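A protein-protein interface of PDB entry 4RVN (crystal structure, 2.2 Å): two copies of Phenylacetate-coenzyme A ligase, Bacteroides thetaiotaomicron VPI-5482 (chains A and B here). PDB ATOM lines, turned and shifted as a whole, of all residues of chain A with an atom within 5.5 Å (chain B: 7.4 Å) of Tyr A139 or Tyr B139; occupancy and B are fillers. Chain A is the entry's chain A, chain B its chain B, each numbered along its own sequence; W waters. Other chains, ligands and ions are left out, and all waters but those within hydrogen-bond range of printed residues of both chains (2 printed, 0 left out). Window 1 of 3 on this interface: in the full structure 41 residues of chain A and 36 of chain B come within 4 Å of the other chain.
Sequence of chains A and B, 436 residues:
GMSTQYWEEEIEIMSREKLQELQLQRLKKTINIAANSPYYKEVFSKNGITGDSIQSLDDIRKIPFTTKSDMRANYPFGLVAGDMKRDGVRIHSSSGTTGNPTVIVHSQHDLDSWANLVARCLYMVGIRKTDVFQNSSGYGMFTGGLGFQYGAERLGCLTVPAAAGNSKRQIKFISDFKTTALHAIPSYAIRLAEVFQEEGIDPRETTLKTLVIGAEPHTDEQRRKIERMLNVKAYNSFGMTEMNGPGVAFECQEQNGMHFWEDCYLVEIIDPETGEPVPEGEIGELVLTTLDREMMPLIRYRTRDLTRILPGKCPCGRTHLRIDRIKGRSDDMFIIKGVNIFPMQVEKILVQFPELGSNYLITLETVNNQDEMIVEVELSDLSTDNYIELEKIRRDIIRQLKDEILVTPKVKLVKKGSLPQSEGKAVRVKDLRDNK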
ATOM      1  N   ASN A 135       5.863  16.251 -24.530  1.00  0.00           N
ATOM      2  CA  ASN A 135       6.827  15.159 -24.638  1.00  0.00           C
ATOM      3  C   ASN A 135       6.135  13.824 -24.329  1.00  0.00           C
ATOM      4  O   ASN A 135       5.748  13.585 -23.185  1.00  0.00           O
ATOM      5  CB  ASN A 135       8.014  15.413 -23.694  1.00  0.00           C
ATOM      6  CG  ASN A 135       9.190  14.493 -23.898  1.00  0.00           C
ATOM      7  OD1 ASN A 135       9.292  13.769 -24.895  1.00  0.00           O
ATOM      8  ND2 ASN A 135      10.143  14.555 -22.983  1.00  0.00           N
ATOM      9  N   SER A 137       7.592  10.908 -24.762  1.00  0.00           N
ATOM     10  CA  SER A 137       8.650   9.946 -24.465  1.00  0.00           C
ATOM     11  C   SER A 137       8.551   9.504 -23.019  1.00  0.00           C
ATOM     12  O   SER A 137       8.126  10.287 -22.170  1.00  0.00           O
ATOM     13  CB  SER A 137      10.023  10.556 -24.741  1.00  0.00           C
ATOM     14  OG  SER A 137      11.078   9.720 -24.285  1.00  0.00           O
ATOM     15  N   GLY A 138       8.969   8.274 -22.745  1.00  0.00           N
ATOM     16  CA  GLY A 138       9.016   7.750 -21.388  1.00  0.00           C
ATOM     17  C   GLY A 138      10.001   8.552 -20.556  1.00  0.00           C
ATOM     18  O   GLY A 138      11.018   9.034 -21.073  1.00  0.00           O
ATOM     19  N   TYR A 139       9.684   8.757 -19.281  1.00  0.00           N
ATOM     20  CA  TYR A 139      10.558   9.525 -18.405  1.00  0.00           C
ATOM     21  C   TYR A 139      11.399   8.531 -17.576  1.00  0.00           C
ATOM     22  O   TYR A 139      11.731   7.456 -18.094  1.00  0.00           O
ATOM     23  CB  TYR A 139       9.735  10.511 -17.556  1.00  0.00           C
ATOM     24  CG  TYR A 139       9.455  11.814 -18.282  1.00  0.00           C
ATOM     25  CD1 TYR A 139       8.644  11.843 -19.414  1.00  0.00           C
ATOM     26  CD2 TYR A 139       9.987  13.018 -17.826  1.00  0.00           C
ATOM     27  CE1 TYR A 139       8.413  13.029 -20.108  1.00  0.00           C
ATOM     28  CE2 TYR A 139       9.739  14.216 -18.494  1.00  0.00           C
ATOM     29  CZ  TYR A 139       8.953  14.216 -19.639  1.00  0.00           C
ATOM     30  OH  TYR A 139       8.710  15.387 -20.313  1.00  0.00           O
ATOM     31  N   GLY A 140      11.796   8.909 -16.362  1.00  0.00           N
ATOM     32  CA  GLY A 140      12.634   8.061 -15.523  1.00  0.00           C
ATOM     33  C   GLY A 140      14.043   7.929 -16.074  1.00  0.00           C
ATOM     34  O   GLY A 140      14.705   8.941 -16.335  1.00  0.00           O
ATOM     35  N   MET A 141      14.493   6.680 -16.296  1.00  0.00           N
ATOM     36  CA  MET A 141      15.841   6.404 -16.797  1.00  0.00           C
ATOM     37  C   MET A 141      15.994   6.720 -18.291  1.00  0.00           C
ATOM     38  O   MET A 141      17.122   6.944 -18.736  1.00  0.00           O
ATOM     39  CB  MET A 141      16.244   4.943 -16.546  1.00  0.00           C
ATOM     40  CG  MET A 141      16.708   4.688 -15.114  1.00  0.00           C
ATOM     41  SD  MET A 141      18.196   5.875 -14.643  1.00  0.00           S
ATOM     42  CE  MET A 141      18.772   4.979 -13.086  1.00  0.00           C
ATOM     43  N   PHE A 142      14.889   6.754 -19.056  1.00  0.00           N
ATOM     44  CA  PHE A 142      14.924   7.074 -20.487  1.00  0.00           C
ATOM     45  C   PHE A 142      15.356   8.522 -20.689  1.00  0.00           C
ATOM     46  O   PHE A 142      14.727   9.430 -20.154  1.00  0.00           O
ATOM     47  CB  PHE A 142      13.566   6.825 -21.152  1.00  0.00           C
ATOM     48  CG  PHE A 142      13.054   5.409 -21.117  1.00  0.00           C
ATOM     49  CD1 PHE A 142      13.584   4.441 -21.957  1.00  0.00           C
ATOM     50  CD2 PHE A 142      11.963   5.068 -20.325  1.00  0.00           C
ATOM     51  CE1 PHE A 142      13.072   3.141 -21.963  1.00  0.00           C
ATOM     52  CE2 PHE A 142      11.448   3.769 -20.334  1.00  0.00           C
ATOM     53  CZ  PHE A 142      12.000   2.817 -21.161  1.00  0.00           C
ATOM     54  N   GLY A 145      12.928  11.557 -21.984  1.00  0.00           N
ATOM     55  CA  GLY A 145      12.041  12.220 -21.037  1.00  0.00           C
ATOM     56  C   GLY A 145      12.652  13.482 -20.466  1.00  0.00           C
ATOM     57  O   GLY A 145      12.264  14.589 -20.858  1.00  0.00           O
ATOM     58  N   LEU A 146      13.628  13.322 -19.556  1.00  0.00           N
ATOM     59  CA  LEU A 146      14.329  14.441 -18.907  1.00  0.00           C
ATOM     60  C   LEU A 146      15.142  15.276 -19.921  1.00  0.00           C
ATOM     61  O   LEU A 146      15.260  16.482 -19.732  1.00  0.00           O
ATOM     62  CB  LEU A 146      15.254  13.947 -17.779  1.00  0.00           C
ATOM     63  CG  LEU A 146      14.569  13.437 -16.494  1.00  0.00           C
ATOM     64  CD1 LEU A 146      15.551  12.695 -15.598  1.00  0.00           C
ATOM     65  CD2 LEU A 146      13.925  14.567 -15.715  1.00  0.00           C
ATOM     66  N   GLN A 149      12.656  17.537 -21.719  1.00  0.00           N
ATOM     67  CA  GLN A 149      12.053  18.347 -20.663  1.00  0.00           C
ATOM     68  C   GLN A 149      12.951  19.548 -20.307  1.00  0.00           C
ATOM     69  O   GLN A 149      12.468  20.683 -20.294  1.00  0.00           O
ATOM     70  CB  GLN A 149      11.772  17.500 -19.403  1.00  0.00           C
ATOM     71  CG  GLN A 149      10.980  18.236 -18.311  1.00  0.00           C
ATOM     72  CD  GLN A 149       9.612  18.662 -18.781  1.00  0.00           C
ATOM     73  OE1 GLN A 149       8.896  17.918 -19.455  1.00  0.00           O
ATOM     74  NE2 GLN A 149       9.214  19.865 -18.421  1.00  0.00           N
ATOM     75  N   VAL A 160       4.629  20.207 -21.486  1.00  0.00           N
ATOM     76  CA  VAL A 160       3.576  19.269 -21.115  1.00  0.00           C
ATOM     77  C   VAL A 160       4.270  17.905 -20.929  1.00  0.00           C
ATOM     78  O   VAL A 160       4.476  17.191 -21.913  1.00  0.00           O
ATOM     79  CB  VAL A 160       2.407  19.247 -22.148  1.00  0.00           C
ATOM     80  CG1 VAL A 160       1.317  18.249 -21.744  1.00  0.00           C
ATOM     81  CG2 VAL A 160       1.813  20.640 -22.346  1.00  0.00           C
ATOM     82  N   PRO A 161       4.717  17.556 -19.698  1.00  0.00           N
ATOM     83  CA  PRO A 161       5.412  16.267 -19.513  1.00  0.00           C
ATOM     84  C   PRO A 161       4.408  15.100 -19.466  1.00  0.00           C
ATOM     85  O   PRO A 161       4.234  14.470 -18.429  1.00  0.00           O
ATOM     86  CB  PRO A 161       6.150  16.463 -18.182  1.00  0.00           C
ATOM     87  CG  PRO A 161       5.306  17.432 -17.419  1.00  0.00           C
ATOM     88  CD  PRO A 161       4.606  18.304 -18.426  1.00  0.00           C
ATOM     89  N   ALA A 162       3.750  14.815 -20.606  1.00  0.00           N
ATOM     90  CA  ALA A 162       2.725  13.777 -20.734  1.00  0.00           C
ATOM     91  C   ALA A 162       3.275  12.369 -20.476  1.00  0.00           C
ATOM     92  O   ALA A 162       2.555  11.532 -19.928  1.00  0.00           O
ATOM     93  CB  ALA A 162       2.110  13.823 -22.124  1.00  0.00           C
ATOM     94  N   ALA A 163       4.536  12.112 -20.879  1.00  0.00           N
ATOM     95  CA  ALA A 163       5.234  10.817 -20.808  1.00  0.00           C
ATOM     96  C   ALA A 163       4.583   9.822 -21.808  1.00  0.00           C
ATOM     97  O   ALA A 163       3.784  10.241 -22.651  1.00  0.00           O
ATOM     98  CB  ALA A 163       5.254  10.255 -19.381  1.00  0.00           C
ATOM     99  N   ALA A 164       4.951   8.530 -21.750  1.00  0.00           N
ATOM    100  CA  ALA A 164       4.487   7.520 -22.702  1.00  0.00           C
ATOM    101  C   ALA A 164       3.021   7.096 -22.488  1.00  0.00           C
ATOM    102  O   ALA A 164       2.493   7.165 -21.382  1.00  0.00           O
ATOM    103  CB  ALA A 164       5.371   6.290 -22.610  1.00  0.00           C
ATOM    104  N   HIS B  92       1.519  20.845 -14.691  1.00  0.00           N
ATOM    105  CA  HIS B  92       1.396  19.610 -13.918  1.00  0.00           C
ATOM    106  C   HIS B  92      -0.082  19.295 -13.706  1.00  0.00           C
ATOM    107  O   HIS B  92      -0.910  20.192 -13.843  1.00  0.00           O
ATOM    108  CB  HIS B  92       2.137  19.680 -12.574  1.00  0.00           C
ATOM    109  CG  HIS B  92       3.589  19.332 -12.664  1.00  0.00           C
ATOM    110  ND1 HIS B  92       4.003  18.024 -12.834  1.00  0.00           N
ATOM    111  CD2 HIS B  92       4.679  20.122 -12.538  1.00  0.00           C
ATOM    112  CE1 HIS B  92       5.325  18.062 -12.847  1.00  0.00           C
ATOM    113  NE2 HIS B  92       5.777  19.301 -12.665  1.00  0.00           N
ATOM    114  N   PHE B 133      20.653   9.825  -4.286  1.00  0.00           N
ATOM    115  CA  PHE B 133      19.207   9.940  -4.115  1.00  0.00           C
ATOM    116  C   PHE B 133      18.447   9.203  -5.220  1.00  0.00           C
ATOM    117  O   PHE B 133      18.605   9.521  -6.394  1.00  0.00           O
ATOM    118  CB  PHE B 133      18.794  11.426  -4.090  1.00  0.00           C
ATOM    119  CG  PHE B 133      17.329  11.671  -3.809  1.00  0.00           C
ATOM    120  CD1 PHE B 133      16.862  11.777  -2.503  1.00  0.00           C
ATOM    121  CD2 PHE B 133      16.415  11.809  -4.851  1.00  0.00           C
ATOM    122  CE1 PHE B 133      15.508  12.002  -2.242  1.00  0.00           C
ATOM    123  CE2 PHE B 133      15.061  12.031  -4.588  1.00  0.00           C
ATOM    124  CZ  PHE B 133      14.619  12.130  -3.285  1.00  0.00           C
ATOM    125  N   GLN B 134      17.586   8.250  -4.832  1.00  0.00           N
ATOM    126  CA  GLN B 134      16.766   7.481  -5.768  1.00  0.00           C
ATOM    127  C   GLN B 134      15.297   7.879  -5.595  1.00  0.00           C
ATOM    128  O   GLN B 134      14.779   7.906  -4.475  1.00  0.00           O
ATOM    129  CB  GLN B 134      16.977   5.972  -5.557  1.00  0.00           C
ATOM    130  CG  GLN B 134      16.316   5.056  -6.588  1.00  0.00           C
ATOM    131  CD  GLN B 134      16.787   3.627  -6.456  1.00  0.00           C
ATOM    132  OE1 GLN B 134      17.975   3.353  -6.247  1.00  0.00           O
ATOM    133  NE2 GLN B 134      15.892   2.678  -6.671  1.00  0.00           N
ATOM    134  N   ASN B 135      14.638   8.211  -6.710  1.00  0.00           N
ATOM    135  CA  ASN B 135      13.237   8.631  -6.707  1.00  0.00           C
ATOM    136  C   ASN B 135      12.371   7.541  -7.353  1.00  0.00           C
ATOM    137  O   ASN B 135      12.476   7.306  -8.560  1.00  0.00           O
ATOM    138  CB  ASN B 135      13.087   9.976  -7.441  1.00  0.00           C
ATOM    139  CG  ASN B 135      11.740  10.639  -7.284  1.00  0.00           C
ATOM    140  OD1 ASN B 135      10.919  10.265  -6.443  1.00  0.00           O
ATOM    141  ND2 ASN B 135      11.515  11.691  -8.049  1.00  0.00           N
ATOM    142  N   SER B 136      11.533   6.859  -6.538  1.00  0.00           N
ATOM    143  CA  SER B 136      10.667   5.782  -7.030  1.00  0.00           C
ATOM    144  C   SER B 136       9.257   6.305  -7.359  1.00  0.00           C
ATOM    145  O   SER B 136       8.349   5.514  -7.619  1.00  0.00           O
ATOM    146  CB  SER B 136      10.579   4.645  -6.015  1.00  0.00           C
ATOM    147  OG  SER B 136       9.811   5.024  -4.888  1.00  0.00           O
ATOM    148  N   SER B 137       9.079   7.632  -7.344  1.00  0.00           N
ATOM    149  CA  SER B 137       7.812   8.258  -7.695  1.00  0.00           C
ATOM    150  C   SER B 137       7.646   8.270  -9.204  1.00  0.00           C
ATOM    151  O   SER B 137       8.640   8.352  -9.925  1.00  0.00           O
ATOM    152  CB  SER B 137       7.745   9.677  -7.137  1.00  0.00           C
ATOM    153  OG  SER B 137       6.613  10.383  -7.626  1.00  0.00           O
ATOM    154  N   GLY B 138       6.397   8.217  -9.663  1.00  0.00           N
ATOM    155  CA  GLY B 138       6.075   8.304 -11.080  1.00  0.00           C
ATOM    156  C   GLY B 138       6.498   9.655 -11.621  1.00  0.00           C
ATOM    157  O   GLY B 138       6.430  10.661 -10.910  1.00  0.00           O
ATOM    158  N   TYR B 139       6.988   9.683 -12.858  1.00  0.00           N
ATOM    159  CA  TYR B 139       7.428  10.936 -13.457  1.00  0.00           C
ATOM    160  C   TYR B 139       6.289  11.454 -14.362  1.00  0.00           C
ATOM    161  O   TYR B 139       5.118  11.246 -14.027  1.00  0.00           O
ATOM    162  CB  TYR B 139       8.774  10.747 -14.183  1.00  0.00           C
ATOM    163  CG  TYR B 139       9.962  10.872 -13.248  1.00  0.00           C
ATOM    164  CD1 TYR B 139      10.185   9.938 -12.241  1.00  0.00           C
ATOM    165  CD2 TYR B 139      10.889  11.898 -13.402  1.00  0.00           C
ATOM    166  CE1 TYR B 139      11.256  10.066 -11.357  1.00  0.00           C
ATOM    167  CE2 TYR B 139      11.984  12.020 -12.543  1.00  0.00           C
ATOM    168  CZ  TYR B 139      12.159  11.104 -11.518  1.00  0.00           C
ATOM    169  OH  TYR B 139      13.218  11.219 -10.654  1.00  0.00           O
ATOM    170  N   GLY B 140       6.612  12.182 -15.422  1.00  0.00           N
ATOM    171  CA  GLY B 140       5.591  12.739 -16.296  1.00  0.00           C
ATOM    172  C   GLY B 140       4.824  13.869 -15.633  1.00  0.00           C
ATOM    173  O   GLY B 140       5.431  14.805 -15.101  1.00  0.00           O
ATOM    174  N   MET B 141       3.478  13.772 -15.651  1.00  0.00           N
ATOM    175  CA  MET B 141       2.570  14.780 -15.090  1.00  0.00           C
ATOM    176  C   MET B 141       2.592  14.781 -13.543  1.00  0.00           C
ATOM    177  O   MET B 141       2.221  15.802 -12.959  1.00  0.00           O
ATOM    178  CB  MET B 141       1.122  14.568 -15.589  1.00  0.00           C
ATOM    179  CG  MET B 141       0.966  14.705 -17.110  1.00  0.00           C
ATOM    180  SD  MET B 141       1.481  16.448 -17.832  1.00  0.00           S
ATOM    181  CE  MET B 141       0.040  17.534 -17.118  1.00  0.00           C
ATOM    182  N   PHE B 142       3.030  13.666 -12.887  1.00  0.00           N
ATOM    183  CA  PHE B 142       3.108  13.538 -11.416  1.00  0.00           C
ATOM    184  C   PHE B 142       4.201  14.444 -10.868  1.00  0.00           C
ATOM    185  O   PHE B 142       5.349  14.330 -11.284  1.00  0.00           O
ATOM    186  CB  PHE B 142       3.355  12.076 -10.966  1.00  0.00           C
ATOM    187  CG  PHE B 142       2.297  11.075 -11.383  1.00  0.00           C
ATOM    188  CD1 PHE B 142       1.043  11.069 -10.780  1.00  0.00           C
ATOM    189  CD2 PHE B 142       2.577  10.100 -12.337  1.00  0.00           C
ATOM    190  CE1 PHE B 142       0.062  10.145 -11.168  1.00  0.00           C
ATOM    191  CE2 PHE B 142       1.606   9.163 -12.710  1.00  0.00           C
ATOM    192  CZ  PHE B 142       0.351   9.197 -12.131  1.00  0.00           C
ATOM    193  N   THR B 143       3.841  15.333  -9.921  1.00  0.00           N
ATOM    194  CA  THR B 143       4.744  16.330  -9.331  1.00  0.00           C
ATOM    195  C   THR B 143       5.877  15.699  -8.508  1.00  0.00           C
ATOM    196  O   THR B 143       6.915  16.332  -8.342  1.00  0.00           O
ATOM    197  CB  THR B 143       3.975  17.307  -8.441  1.00  0.00           C
ATOM    198  OG1 THR B 143       3.455  16.622  -7.302  1.00  0.00           O
ATOM    199  CG2 THR B 143       2.884  18.041  -9.191  1.00  0.00           C
ATOM    200  N   GLY B 144       5.669  14.485  -8.001  1.00  0.00           N
ATOM    201  CA  GLY B 144       6.668  13.777  -7.210  1.00  0.00           C
ATOM    202  C   GLY B 144       7.928  13.423  -7.979  1.00  0.00           C
ATOM    203  O   GLY B 144       9.014  13.361  -7.394  1.00  0.00           O
ATOM    204  N   GLY B 145       7.780  13.189  -9.287  1.00  0.00           N
ATOM    205  CA  GLY B 145       8.872  12.836 -10.184  1.00  0.00           C
ATOM    206  C   GLY B 145       9.824  13.986 -10.414  1.00  0.00           C
ATOM    207  O   GLY B 145      10.926  13.997  -9.861  1.00  0.00           O
ATOM    208  N   LEU B 146       9.388  14.978 -11.208  1.00  0.00           N
ATOM    209  CA  LEU B 146      10.194  16.163 -11.531  1.00  0.00           C
ATOM    210  C   LEU B 146      10.457  17.033 -10.281  1.00  0.00           C
ATOM    211  O   LEU B 146      11.502  17.681 -10.215  1.00  0.00           O
ATOM    212  CB  LEU B 146       9.516  17.007 -12.625  1.00  0.00           C
ATOM    213  CG  LEU B 146       9.513  16.424 -14.057  1.00  0.00           C
ATOM    214  CD1 LEU B 146       8.551  17.167 -14.954  1.00  0.00           C
ATOM    215  CD2 LEU B 146      10.899  16.441 -14.678  1.00  0.00           C
ATOM    216  N   GLY B 147       9.537  17.009  -9.308  1.00  0.00           N
ATOM    217  CA  GLY B 147       9.661  17.755  -8.052  1.00  0.00           C
ATOM    218  C   GLY B 147      10.879  17.390  -7.232  1.00  0.00           C
ATOM    219  O   GLY B 147      11.675  18.265  -6.885  1.00  0.00           O
ATOM    220  N   PHE B 148      11.051  16.091  -6.934  1.00  0.00           N
ATOM    221  CA  PHE B 148      12.223  15.627  -6.193  1.00  0.00           C
ATOM    222  C   PHE B 148      13.464  15.586  -7.084  1.00  0.00           C
ATOM    223  O   PHE B 148      14.564  15.782  -6.570  1.00  0.00           O
ATOM    224  CB  PHE B 148      11.991  14.251  -5.557  1.00  0.00           C
ATOM    225  CG  PHE B 148      11.300  14.335  -4.213  1.00  0.00           C
ATOM    226  CD1 PHE B 148      12.002  14.719  -3.075  1.00  0.00           C
ATOM    227  CD2 PHE B 148       9.962  13.997  -4.080  1.00  0.00           C
ATOM    228  CE1 PHE B 148      11.361  14.804  -1.831  1.00  0.00           C
ATOM    229  CE2 PHE B 148       9.330  14.058  -2.833  1.00  0.00           C
ATOM    230  CZ  PHE B 148      10.030  14.471  -1.719  1.00  0.00           C
ATOM    231  N   GLN B 149      13.299  15.367  -8.405  1.00  0.00           N
ATOM    232  CA  GLN B 149      14.420  15.329  -9.349  1.00  0.00           C
ATOM    233  C   GLN B 149      15.167  16.670  -9.363  1.00  0.00           C
ATOM    234  O   GLN B 149      16.389  16.678  -9.219  1.00  0.00           O
ATOM    235  CB  GLN B 149      13.937  14.970 -10.772  1.00  0.00           C
ATOM    236  CG  GLN B 149      15.075  14.748 -11.777  1.00  0.00           C
ATOM    237  CD  GLN B 149      15.978  13.596 -11.394  1.00  0.00           C
ATOM    238  OE1 GLN B 149      15.530  12.535 -10.942  1.00  0.00           O
ATOM    239  NE2 GLN B 149      17.277  13.779 -11.572  1.00  0.00           N
ATOM    240  N   TYR B 150      14.437  17.788  -9.527  1.00  0.00           N
ATOM    241  CA  TYR B 150      15.005  19.141  -9.564  1.00  0.00           C
ATOM    242  C   TYR B 150      15.553  19.553  -8.203  1.00  0.00           C
ATOM    243  O   TYR B 150      16.618  20.162  -8.152  1.00  0.00           O
ATOM    244  CB  TYR B 150      13.956  20.161 -10.034  1.00  0.00           C
ATOM    245  CG  TYR B 150      13.792  20.222 -11.538  1.00  0.00           C
ATOM    246  CD1 TYR B 150      13.435  19.089 -12.267  1.00  0.00           C
ATOM    247  CD2 TYR B 150      13.880  21.435 -12.219  1.00  0.00           C
ATOM    248  CE1 TYR B 150      13.241  19.146 -13.642  1.00  0.00           C
ATOM    249  CE2 TYR B 150      13.692  21.503 -13.601  1.00  0.00           C
ATOM    250  CZ  TYR B 150      13.392  20.350 -14.310  1.00  0.00           C
ATOM    251  OH  TYR B 150      13.185  20.396 -15.666  1.00  0.00           O
ATOM    252  N   THR B 159      21.611  11.765  -8.405  1.00  0.00           N
ATOM    253  CA  THR B 159      20.221  11.307  -8.525  1.00  0.00           C
ATOM    254  C   THR B 159      20.114  10.053  -9.387  1.00  0.00           C
ATOM    255  O   THR B 159      20.888   9.849 -10.325  1.00  0.00           O
ATOM    256  CB  THR B 159      19.293  12.399  -9.085  1.00  0.00           C
ATOM    257  OG1 THR B 159      19.621  12.677 -10.449  1.00  0.00           O
ATOM    258  CG2 THR B 159      19.316  13.669  -8.256  1.00  0.00           C
ATOM    259  N   VAL B 160      19.125   9.215  -9.039  1.00  0.00           N
ATOM    260  CA  VAL B 160      18.777   7.964  -9.703  1.00  0.00           C
ATOM    261  C   VAL B 160      17.290   8.083 -10.070  1.00  0.00           C
ATOM    262  O   VAL B 160      16.432   7.806  -9.225  1.00  0.00           O
ATOM    263  CB  VAL B 160      19.121   6.711  -8.828  1.00  0.00           C
ATOM    264  CG1 VAL B 160      18.749   5.412  -9.536  1.00  0.00           C
ATOM    265  CG2 VAL B 160      20.597   6.686  -8.432  1.00  0.00           C
ATOM    266  N   PRO B 161      16.949   8.585 -11.286  1.00  0.00           N
ATOM    267  CA  PRO B 161      15.521   8.742 -11.635  1.00  0.00           C
ATOM    268  C   PRO B 161      14.906   7.392 -12.032  1.00  0.00           C
ATOM    269  O   PRO B 161      14.563   7.174 -13.192  1.00  0.00           O
ATOM    270  CB  PRO B 161      15.554   9.736 -12.800  1.00  0.00           C
ATOM    271  CG  PRO B 161      16.890   9.503 -13.458  1.00  0.00           C
ATOM    272  CD  PRO B 161      17.835   9.016 -12.392  1.00  0.00           C
ATOM    273  N   ALA B 162      14.771   6.482 -11.058  1.00  0.00           N
ATOM    274  CA  ALA B 162      14.255   5.126 -11.267  1.00  0.00           C
ATOM    275  C   ALA B 162      12.795   5.115 -11.738  1.00  0.00           C
ATOM    276  O   ALA B 162      12.427   4.240 -12.528  1.00  0.00           O
ATOM    277  CB  ALA B 162      14.368   4.327  -9.978  1.00  0.00           C
ATOM    278  N   ALA B 163      11.972   6.084 -11.247  1.00  0.00           N
ATOM    279  CA  ALA B 163      10.527   6.222 -11.493  1.00  0.00           C
ATOM    280  C   ALA B 163       9.773   5.062 -10.802  1.00  0.00           C
ATOM    281  O   ALA B 163      10.373   4.342 -10.002  1.00  0.00           O
ATOM    282  CB  ALA B 163      10.207   6.289 -12.989  1.00  0.00           C
ATOM    283  N   ALA B 164       8.468   4.907 -11.070  1.00  0.00           N
ATOM    284  CA  ALA B 164       7.621   3.909 -10.410  1.00  0.00           C
ATOM    285  C   ALA B 164       7.880   2.472 -10.889  1.00  0.00           C
ATOM    286  O   ALA B 164       8.293   2.241 -12.025  1.00  0.00           O
ATOM    287  CB  ALA B 164       6.155   4.244 -10.643  1.00  0.00           C
ATOM    288  N   ARG B 169      14.624  -4.004 -10.385  1.00  0.00           N
ATOM    289  CA  ARG B 169      15.504  -2.976 -10.944  1.00  0.00           C
ATOM    290  C   ARG B 169      15.818  -1.923  -9.862  1.00  0.00           C
ATOM    291  O   ARG B 169      16.945  -1.432  -9.811  1.00  0.00           O
ATOM    292  CB  ARG B 169      14.856  -2.339 -12.184  1.00  0.00           C
ATOM    293  CG  ARG B 169      15.840  -1.624 -13.094  1.00  0.00           C
ATOM    294  CD  ARG B 169      15.137  -1.026 -14.291  1.00  0.00           C
ATOM    295  NE  ARG B 169      16.077  -0.313 -15.147  1.00  0.00           N
ATOM    296  CZ  ARG B 169      15.723   0.612 -16.032  1.00  0.00           C
ATOM    297  NH1 ARG B 169      14.453   0.971 -16.155  1.00  0.00           N
ATOM    298  NH2 ARG B 169      16.642   1.213 -16.776  1.00  0.00           N
HETATM  299  O   HOH W   1      13.062   4.486 -15.200  1.00  0.00           O
HETATM  300  O   HOH W   2       2.115  11.485 -17.005  1.00  0.00           O
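O of Asn A135 sits at hydrogen-bond distance from N of Ala A163, at 3.0 Å.
ND2 of Asn B135 is in hydrogen-bond range of OH of Tyr B139 (3.1 Å).
N of Ala B163 sits at hydrogen-bond distance from O of Asn B135 (3.0 Å).
The side-chain amide nitrogen of Asn A135 is in hydrogen-bond range of the side-chain hydroxyl of Tyr A139 (3.1 Å).
The side-chain hydroxyl (OH) of Tyr B139 is in hydrogen-bond range of the side-chain amide oxygen (OE1) of Gln B149 (2.7 Å).
N of Asn B135 is in hydrogen-bond range of O of Val B160 (3.1 Å).
Of the 26 printed residues of chain B, 8 touch a printed residue of chain A.
Hydrophobic or aromatic side chains of chain B that line the printed part of chain A: Tyr B139, Met B141, Leu B146, Val B160, Pro B161 and Ala B163.
Hydrophobic or aromatic side chains of chain A that line the printed part of chain B: Tyr A139, Met A141, Leu A146, Pro A161 and Ala A163.
Along chain A the printed residues that touch a printed residue of chain B span positions 139 to 163.
Among the printed residues, 11 pairs touch across the chains.
Among the printed residues, no Asp or Glu carboxylate lies within 4 Å of a Lys or Arg side-chain nitrogen of the other chain.
Gly A140 touches Pro B161, and with the chains exchanged Pro A161 touches Gly B140.
Gly A140 touches Ala B163, and with the chains exchanged Ala A163 touches Gly B140.
Leu B146 touches its own counterpart, Leu A146.
Ala A162 touches Met B141, but with the chains exchanged Met A141 does not touch Ala B162 (4.6 Å).
15 positions are printed for both chains.
Of the 11 pairs that touch across the chains among the printed residues, 8 have their exchanged pair printed and touching as well.
Of chain B, only Tyr B139 comes within 4 Å of Tyr A139.
Of the printed residues of chain B, Met A141 touches Val B160 (3.6 Å), Pro B161 (3.1 Å) and Arg B169 (3.8 Å).
Tyr B139 touches just one residue of chain A: Tyr A139.
Of the printed residues of chain A, Gly B140 touches Pro A161 and Ala A163.
Gly B145 touches none of the printed residues of chain A.
Phe B148 touches none of the printed residues of chain A.
The nearest residue of chain B that does not touch Tyr A139 is Gly B140 (4.05 Å).
Tyr B139 touches Tyr A139.
Gly A140 touches Pro B161 (C to O, 3.0 Å).
Ala B163 touches Gly A140.
Met A141 touches Val B160.
Arg B169 touches Met A141.
CD2 of Leu A146 touches CD2 of Leu B146 (3.7 Å).
Pro A161 touches Gly B140 (O to C, 2.9 Å).
Met B141 touches Ala A162.
Ala A163 touches Gly B140.
Water W1 lies within hydrogen-bond range of the backbone carbonyl oxygen of Ala B162 (2.8 Å) and the backbone NH of Met A141 (2.8 Å).
Water W2 bridges the backbone carbonyl oxygen of Ala A162 (3.0 Å) and the backbone NH of Met B141 (3.0 Å).
N of Met A141 sits at hydrogen-bond distance from O of Pro B161 (3.1 Å).
O of Pro A161 is in hydrogen-bond range of N of Met B141.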
